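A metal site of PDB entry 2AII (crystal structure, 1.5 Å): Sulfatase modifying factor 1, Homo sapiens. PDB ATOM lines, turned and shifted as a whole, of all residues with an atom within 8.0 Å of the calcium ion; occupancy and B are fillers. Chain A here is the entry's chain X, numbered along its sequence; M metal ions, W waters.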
ATOM      1  N   HIS A 171       9.957 -15.745  31.066  1.00  0.00           N
ATOM      2  CA  HIS A 171      11.367 -15.499  31.350  1.00  0.00           C
ATOM      3  C   HIS A 171      11.644 -15.557  32.843  1.00  0.00           C
ATOM      4  O   HIS A 171      10.887 -14.966  33.641  1.00  0.00           O
ATOM      5  CB  HIS A 171      11.831 -14.169  30.742  1.00  0.00           C
ATOM      6  CG  HIS A 171      12.051 -14.254  29.269  1.00  0.00           C
ATOM      7  ND1 HIS A 171      13.145 -14.900  28.730  1.00  0.00           N
ATOM      8  CD2 HIS A 171      11.292 -13.864  28.214  1.00  0.00           C
ATOM      9  CE1 HIS A 171      13.064 -14.889  27.418  1.00  0.00           C
ATOM     10  NE2 HIS A 171      11.946 -14.259  27.075  1.00  0.00           N
ATOM     11  N   ALA A 173      15.117 -15.278  34.051  1.00  0.00           N
ATOM     12  CA  ALA A 173      16.413 -14.650  34.291  1.00  0.00           C
ATOM     13  C   ALA A 173      16.751 -13.709  33.180  1.00  0.00           C
ATOM     14  O   ALA A 173      16.245 -13.834  32.061  1.00  0.00           O
ATOM     15  CB  ALA A 173      17.520 -15.678  34.439  1.00  0.00           C
ATOM     16  N   ASN A 174      17.633 -12.765  33.484  1.00  0.00           N
ATOM     17  CA  ASN A 174      18.090 -11.780  32.510  1.00  0.00           C
ATOM     18  C   ASN A 174      19.380 -12.228  31.840  1.00  0.00           C
ATOM     19  O   ASN A 174      20.456 -12.115  32.395  1.00  0.00           O
ATOM     20  CB  ASN A 174      18.305 -10.430  33.196  1.00  0.00           C
ATOM     21  CG  ASN A 174      18.796  -9.366  32.262  1.00  0.00           C
ATOM     22  OD1 ASN A 174      18.631  -9.474  31.056  1.00  0.00           O
ATOM     23  ND2 ASN A 174      19.406  -8.301  32.812  1.00  0.00           N
ATOM     24  N   ILE A 175      19.249 -12.778  30.630  1.00  0.00           N
ATOM     25  CA  ILE A 175      20.364 -13.176  29.786  1.00  0.00           C
ATOM     26  C   ILE A 175      20.149 -12.512  28.389  1.00  0.00           C
ATOM     27  O   ILE A 175      19.391 -11.546  28.261  1.00  0.00           O
ATOM     28  CB  ILE A 175      20.503 -14.728  29.753  1.00  0.00           C
ATOM     29  CG1 ILE A 175      19.250 -15.405  29.213  1.00  0.00           C
ATOM     30  CG2 ILE A 175      20.765 -15.240  31.152  1.00  0.00           C
ATOM     31  CD1 ILE A 175      19.484 -16.857  28.824  1.00  0.00           C
ATOM     32  N   TRP A 176      20.804 -13.029  27.359  1.00  0.00           N
ATOM     33  CA  TRP A 176      20.732 -12.430  26.030  1.00  0.00           C
ATOM     34  C   TRP A 176      19.709 -13.150  25.181  1.00  0.00           C
ATOM     35  O   TRP A 176      19.627 -14.371  25.243  1.00  0.00           O
ATOM     36  CB  TRP A 176      22.082 -12.618  25.352  1.00  0.00           C
ATOM     37  CG  TRP A 176      22.297 -11.935  24.042  1.00  0.00           C
ATOM     38  CD1 TRP A 176      21.870 -12.346  22.812  1.00  0.00           C
ATOM     39  CD2 TRP A 176      23.068 -10.745  23.816  1.00  0.00           C
ATOM     40  NE1 TRP A 176      22.306 -11.470  21.842  1.00  0.00           N
ATOM     41  CE2 TRP A 176      23.040 -10.477  22.436  1.00  0.00           C
ATOM     42  CE3 TRP A 176      23.759  -9.872  24.662  1.00  0.00           C
ATOM     43  CZ2 TRP A 176      23.694  -9.379  21.875  1.00  0.00           C
ATOM     44  CZ3 TRP A 176      24.409  -8.798  24.107  1.00  0.00           C
ATOM     45  CH2 TRP A 176      24.377  -8.554  22.732  1.00  0.00           C
ATOM     46  N   GLN A 177      18.941 -12.399  24.393  1.00  0.00           N
ATOM     47  CA  GLN A 177      18.160 -12.999  23.309  1.00  0.00           C
ATOM     48  C   GLN A 177      18.574 -12.285  22.045  1.00  0.00           C
ATOM     49  O   GLN A 177      18.816 -11.087  22.068  1.00  0.00           O
ATOM     50  CB  GLN A 177      16.655 -12.856  23.522  1.00  0.00           C
ATOM     51  CG  GLN A 177      16.122 -13.582  24.748  1.00  0.00           C
ATOM     52  CD  GLN A 177      16.220 -12.740  25.988  1.00  0.00           C
ATOM     53  OE1 GLN A 177      16.000 -11.525  25.937  1.00  0.00           O
ATOM     54  NE2 GLN A 177      16.575 -13.371  27.129  1.00  0.00           N
ATOM     55  N   ASN A 184      20.892  -7.686  20.623  1.00  0.00           N
ATOM     56  CA  ASN A 184      20.189  -8.131  21.811  1.00  0.00           C
ATOM     57  C   ASN A 184      18.776  -7.602  21.683  1.00  0.00           C
ATOM     58  O   ASN A 184      18.564  -6.408  21.726  1.00  0.00           O
ATOM     59  CB  ASN A 184      20.844  -7.565  23.098  1.00  0.00           C
ATOM     60  CG  ASN A 184      20.264  -8.169  24.360  1.00  0.00           C
ATOM     61  OD1 ASN A 184      19.160  -8.715  24.350  1.00  0.00           O
ATOM     62  ND2 ASN A 184      21.015  -8.102  25.465  1.00  0.00           N
ATOM     63  N   THR A 185      17.806  -8.493  21.520  1.00  0.00           N
ATOM     64  CA  THR A 185      16.446  -8.057  21.275  1.00  0.00           C
ATOM     65  C   THR A 185      15.748  -7.481  22.490  1.00  0.00           C
ATOM     66  O   THR A 185      14.743  -6.783  22.362  1.00  0.00           O
ATOM     67  CB  THR A 185      15.601  -9.229  20.780  1.00  0.00           C
ATOM     68  OG1 THR A 185      15.489 -10.195  21.821  1.00  0.00           O
ATOM     69  CG2 THR A 185      16.213  -9.877  19.548  1.00  0.00           C
ATOM     70  N   GLY A 186      16.283  -7.746  23.694  1.00  0.00           N
ATOM     71  CA  GLY A 186      15.647  -7.296  24.929  1.00  0.00           C
ATOM     72  C   GLY A 186      14.290  -7.934  25.165  1.00  0.00           C
ATOM     73  O   GLY A 186      13.439  -7.383  25.864  1.00  0.00           O
ATOM     74  N   GLU A 187      14.116  -9.125  24.609  1.00  0.00           N
ATOM     75  CA  GLU A 187      12.875  -9.875  24.766  1.00  0.00           C
ATOM     76  C   GLU A 187      12.499 -10.074  26.244  1.00  0.00           C
ATOM     77  O   GLU A 187      11.311  -9.977  26.594  1.00  0.00           O
ATOM     78  CB  GLU A 187      13.004 -11.242  24.071  1.00  0.00           C
ATOM     79  CG  GLU A 187      11.779 -12.146  24.186  1.00  0.00           C
ATOM     80  CD  GLU A 187      12.049 -13.545  23.729  1.00  0.00           C
ATOM     81  OE1 GLU A 187      12.887 -13.735  22.823  1.00  0.00           O
ATOM     82  OE2 GLU A 187      11.390 -14.470  24.270  1.00  0.00           O
ATOM     83  N   ASP A 188      13.494 -10.360  27.102  1.00  0.00           N
ATOM     84  CA  ASP A 188      13.225 -10.604  28.534  1.00  0.00           C
ATOM     85  C   ASP A 188      12.964  -9.334  29.344  1.00  0.00           C
ATOM     86  O   ASP A 188      12.733  -9.414  30.549  1.00  0.00           O
ATOM     87  CB  ASP A 188      14.303 -11.435  29.206  1.00  0.00           C
ATOM     88  CG  ASP A 188      15.661 -10.755  29.204  1.00  0.00           C
ATOM     89  OD1 ASP A 188      15.726  -9.495  29.079  1.00  0.00           O
ATOM     90  OD2 ASP A 188      16.687 -11.492  29.300  1.00  0.00           O
ATOM     91  N   GLY A 189      12.991  -8.184  28.677  1.00  0.00           N
ATOM     92  CA  GLY A 189      12.710  -6.907  29.295  1.00  0.00           C
ATOM     93  C   GLY A 189      13.893  -6.019  29.600  1.00  0.00           C
ATOM     94  O   GLY A 189      13.714  -4.873  29.994  1.00  0.00           O
ATOM     95  N   PHE A 190      15.105  -6.546  29.408  1.00  0.00           N
ATOM     96  CA  PHE A 190      16.333  -5.829  29.772  1.00  0.00           C
ATOM     97  C   PHE A 190      17.455  -6.148  28.823  1.00  0.00           C
ATOM     98  O   PHE A 190      17.793  -7.318  28.638  1.00  0.00           O
ATOM     99  CB  PHE A 190      16.740  -6.178  31.202  1.00  0.00           C
ATOM    100  CG  PHE A 190      15.652  -5.961  32.187  1.00  0.00           C
ATOM    101  CD1 PHE A 190      15.453  -4.713  32.741  1.00  0.00           C
ATOM    102  CD2 PHE A 190      14.775  -6.980  32.521  1.00  0.00           C
ATOM    103  CE1 PHE A 190      14.390  -4.469  33.604  1.00  0.00           C
ATOM    104  CE2 PHE A 190      13.729  -6.758  33.396  1.00  0.00           C
ATOM    105  CZ  PHE A 190      13.546  -5.504  33.945  1.00  0.00           C
ATOM    106  N   GLN A 191      18.020  -5.115  28.210  1.00  0.00           N
ATOM    107  CA  GLN A 191      19.215  -5.302  27.388  1.00  0.00           C
ATOM    108  C   GLN A 191      20.472  -5.380  28.236  1.00  0.00           C
ATOM    109  O   GLN A 191      21.287  -6.311  28.089  1.00  0.00           O
ATOM    110  CB  GLN A 191      19.292  -4.199  26.356  1.00  0.00           C
ATOM    111  CG  GLN A 191      18.242  -4.430  25.307  1.00  0.00           C
ATOM    112  CD  GLN A 191      18.149  -3.332  24.314  1.00  0.00           C
ATOM    113  OE1 GLN A 191      18.111  -2.174  24.682  1.00  0.00           O
ATOM    114  NE2 GLN A 191      18.064  -3.694  23.027  1.00  0.00           N
ATOM    115  N   GLY A 192      20.629  -4.414  29.147  1.00  0.00           N
ATOM    116  CA  GLY A 192      21.688  -4.472  30.122  1.00  0.00           C
ATOM    117  C   GLY A 192      21.140  -5.108  31.387  1.00  0.00           C
ATOM    118  O   GLY A 192      20.373  -6.063  31.321  1.00  0.00           O
ATOM    119  N   THR A 193      21.509  -4.545  32.538  1.00  0.00           N
ATOM    120  CA  THR A 193      21.075  -5.064  33.801  1.00  0.00           C
ATOM    121  C   THR A 193      19.594  -4.763  34.041  1.00  0.00           C
ATOM    122  O   THR A 193      19.006  -3.901  33.369  1.00  0.00           O
ATOM    123  CB  THR A 193      21.917  -4.482  34.965  1.00  0.00           C
ATOM    124  OG1 THR A 193      21.858  -3.060  34.908  1.00  0.00           O
ATOM    125  CG2 THR A 193      23.361  -4.969  34.861  1.00  0.00           C
ATOM    126  N   ALA A 194      19.043  -5.556  34.966  1.00  0.00           N
ATOM    127  CA  ALA A 194      17.710  -5.387  35.531  1.00  0.00           C
ATOM    128  C   ALA A 194      17.849  -5.015  36.992  1.00  0.00           C
ATOM    129  O   ALA A 194      18.895  -5.267  37.616  1.00  0.00           O
ATOM    130  CB  ALA A 194      16.933  -6.690  35.443  1.00  0.00           C
ATOM    131  N   PHE A 199      12.551 -10.580  38.201  1.00  0.00           N
ATOM    132  CA  PHE A 199      12.397 -12.022  37.900  1.00  0.00           C
ATOM    133  C   PHE A 199      11.989 -12.827  39.136  1.00  0.00           C
ATOM    134  O   PHE A 199      12.068 -12.333  40.241  1.00  0.00           O
ATOM    135  CB  PHE A 199      13.626 -12.549  37.170  1.00  0.00           C
ATOM    136  CG  PHE A 199      13.790 -11.923  35.808  1.00  0.00           C
ATOM    137  CD1 PHE A 199      12.955 -12.276  34.763  1.00  0.00           C
ATOM    138  CD2 PHE A 199      14.714 -10.912  35.616  1.00  0.00           C
ATOM    139  CE1 PHE A 199      13.083 -11.648  33.533  1.00  0.00           C
ATOM    140  CE2 PHE A 199      14.820 -10.272  34.406  1.00  0.00           C
ATOM    141  CZ  PHE A 199      14.025 -10.648  33.362  1.00  0.00           C
ATOM    142  N   ASN A 212      21.863 -11.580  34.933  1.00  0.00           N
ATOM    143  CA  ASN A 212      21.962 -10.198  35.401  1.00  0.00           C
ATOM    144  C   ASN A 212      23.430  -9.837  35.541  1.00  0.00           C
ATOM    145  O   ASN A 212      24.059  -9.618  34.513  1.00  0.00           O
ATOM    146  CB  ASN A 212      21.077  -9.925  36.623  1.00  0.00           C
ATOM    147  CG  ASN A 212      20.503  -8.509  36.611  1.00  0.00           C
ATOM    148  OD1 ASN A 212      20.245  -7.952  35.547  1.00  0.00           O
ATOM    149  ND2 ASN A 212      20.243  -7.955  37.792  1.00  0.00           N
ATOM    150  N   SER A 248      25.507 -13.743  33.284  1.00  0.00           N
ATOM    151  CA  SER A 248      25.070 -12.369  33.222  1.00  0.00           C
ATOM    152  C   SER A 248      24.073 -12.119  32.094  1.00  0.00           C
ATOM    153  O   SER A 248      23.688 -13.038  31.343  1.00  0.00           O
ATOM    154  CB  SER A 248      26.285 -11.462  33.012  1.00  0.00           C
ATOM    155  OG  SER A 248      26.724 -11.512  31.663  1.00  0.00           O
ATOM    156  N   TYR A 249      23.708 -10.866  31.963  1.00  0.00           N
ATOM    157  CA  TYR A 249      22.806 -10.409  30.912  1.00  0.00           C
ATOM    158  C   TYR A 249      23.352 -10.632  29.508  1.00  0.00           C
ATOM    159  O   TYR A 249      22.610 -10.517  28.519  1.00  0.00           O
ATOM    160  CB  TYR A 249      22.467  -8.930  31.108  1.00  0.00           C
ATOM    161  CG  TYR A 249      23.589  -7.936  30.930  1.00  0.00           C
ATOM    162  CD1 TYR A 249      24.214  -7.364  32.036  1.00  0.00           C
ATOM    163  CD2 TYR A 249      23.980  -7.529  29.664  1.00  0.00           C
ATOM    164  CE1 TYR A 249      25.228  -6.429  31.862  1.00  0.00           C
ATOM    165  CE2 TYR A 249      24.987  -6.589  29.494  1.00  0.00           C
ATOM    166  CZ  TYR A 249      25.595  -6.049  30.593  1.00  0.00           C
ATOM    167  OH  TYR A 249      26.607  -5.101  30.445  1.00  0.00           O
ATOM    168  N   MET A 250      24.645 -10.945  29.408  1.00  0.00           N
ATOM    169  CA  MET A 250      25.294 -11.214  28.123  1.00  0.00           C
ATOM    170  C   MET A 250      25.223 -12.663  27.654  1.00  0.00           C
ATOM    171  O   MET A 250      25.568 -12.954  26.501  1.00  0.00           O
ATOM    172  CB  MET A 250      26.773 -10.816  28.203  1.00  0.00           C
ATOM    173  CG  MET A 250      26.989  -9.343  28.242  1.00  0.00           C
ATOM    174  SD  MET A 250      28.701  -8.952  28.604  1.00  0.00           S
ATOM    175  CE  MET A 250      29.473  -9.400  27.054  1.00  0.00           C
ATOM    176  N   CYS A 251      24.840 -13.594  28.528  1.00  0.00           N
ATOM    177  CA  CYS A 251      24.960 -15.015  28.170  1.00  0.00           C
ATOM    178  C   CYS A 251      23.940 -15.508  27.161  1.00  0.00           C
ATOM    179  O   CYS A 251      22.789 -15.142  27.203  1.00  0.00           O
ATOM    180  CB  CYS A 251      24.824 -15.910  29.384  1.00  0.00           C
ATOM    181  SG  CYS A 251      26.039 -15.684  30.673  1.00  0.00           S
HETATM  182 CA    CA M   1      18.189  -9.604  28.795  1.00  0.00          CA
HETATM  183  O   HOH W   1      17.697  -9.585  26.426  1.00  0.00           O
HETATM  184  O   HOH W   2      20.410  -8.865  28.251  1.00  0.00           O
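The side-chain amide nitrogen (ND2) of Asn 174 sits at hydrogen-bond distance from the side-chain amide oxygen (OD1) of Asn 212, 2.9 Å away. The side-chain amide oxygen of Gln 177 sits at hydrogen-bond distance from the backbone NH of Asp 188 (3.0 Å). The side-chain amide nitrogen (ND2) of Asn 174 is in hydrogen-bond range of the backbone carbonyl oxygen (O) of Gly 192, 2.9 Å away.
Four residues have an atom within 4 Å of the calcium ion: Asn 174, Ile 175, Asp 188 and Phe 190.
OD1 of Asn 174 binds the calcium ion. O of Phe 190 binds the calcium ion (2.3 Å). O of Ile 175 binds the calcium ion, 2.3 Å away. Water W2 binds the calcium ion. Water W1 is bound to the calcium ion, 2.4 Å away. The calcium ion is bound by OD2 of Asp 188 (2.5 Å). The side-chain carboxylate (OD1) of Asp 188 binds the calcium ion, 2.5 Å away. The calcium ion has seven donor atoms within binding distance.
Water W1 lies within hydrogen-bond range of the side-chain amide oxygen (OE1) of Gln 177 (2.6 Å) and the side-chain amide oxygen (OD1) of Asn 184 (2.7 Å). Water W2 lies within hydrogen-bond range of O of Gln 191 (2.7 Å), O of Tyr 249 (2.8 Å) and ND2 of Asn 184 (3.0 Å).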
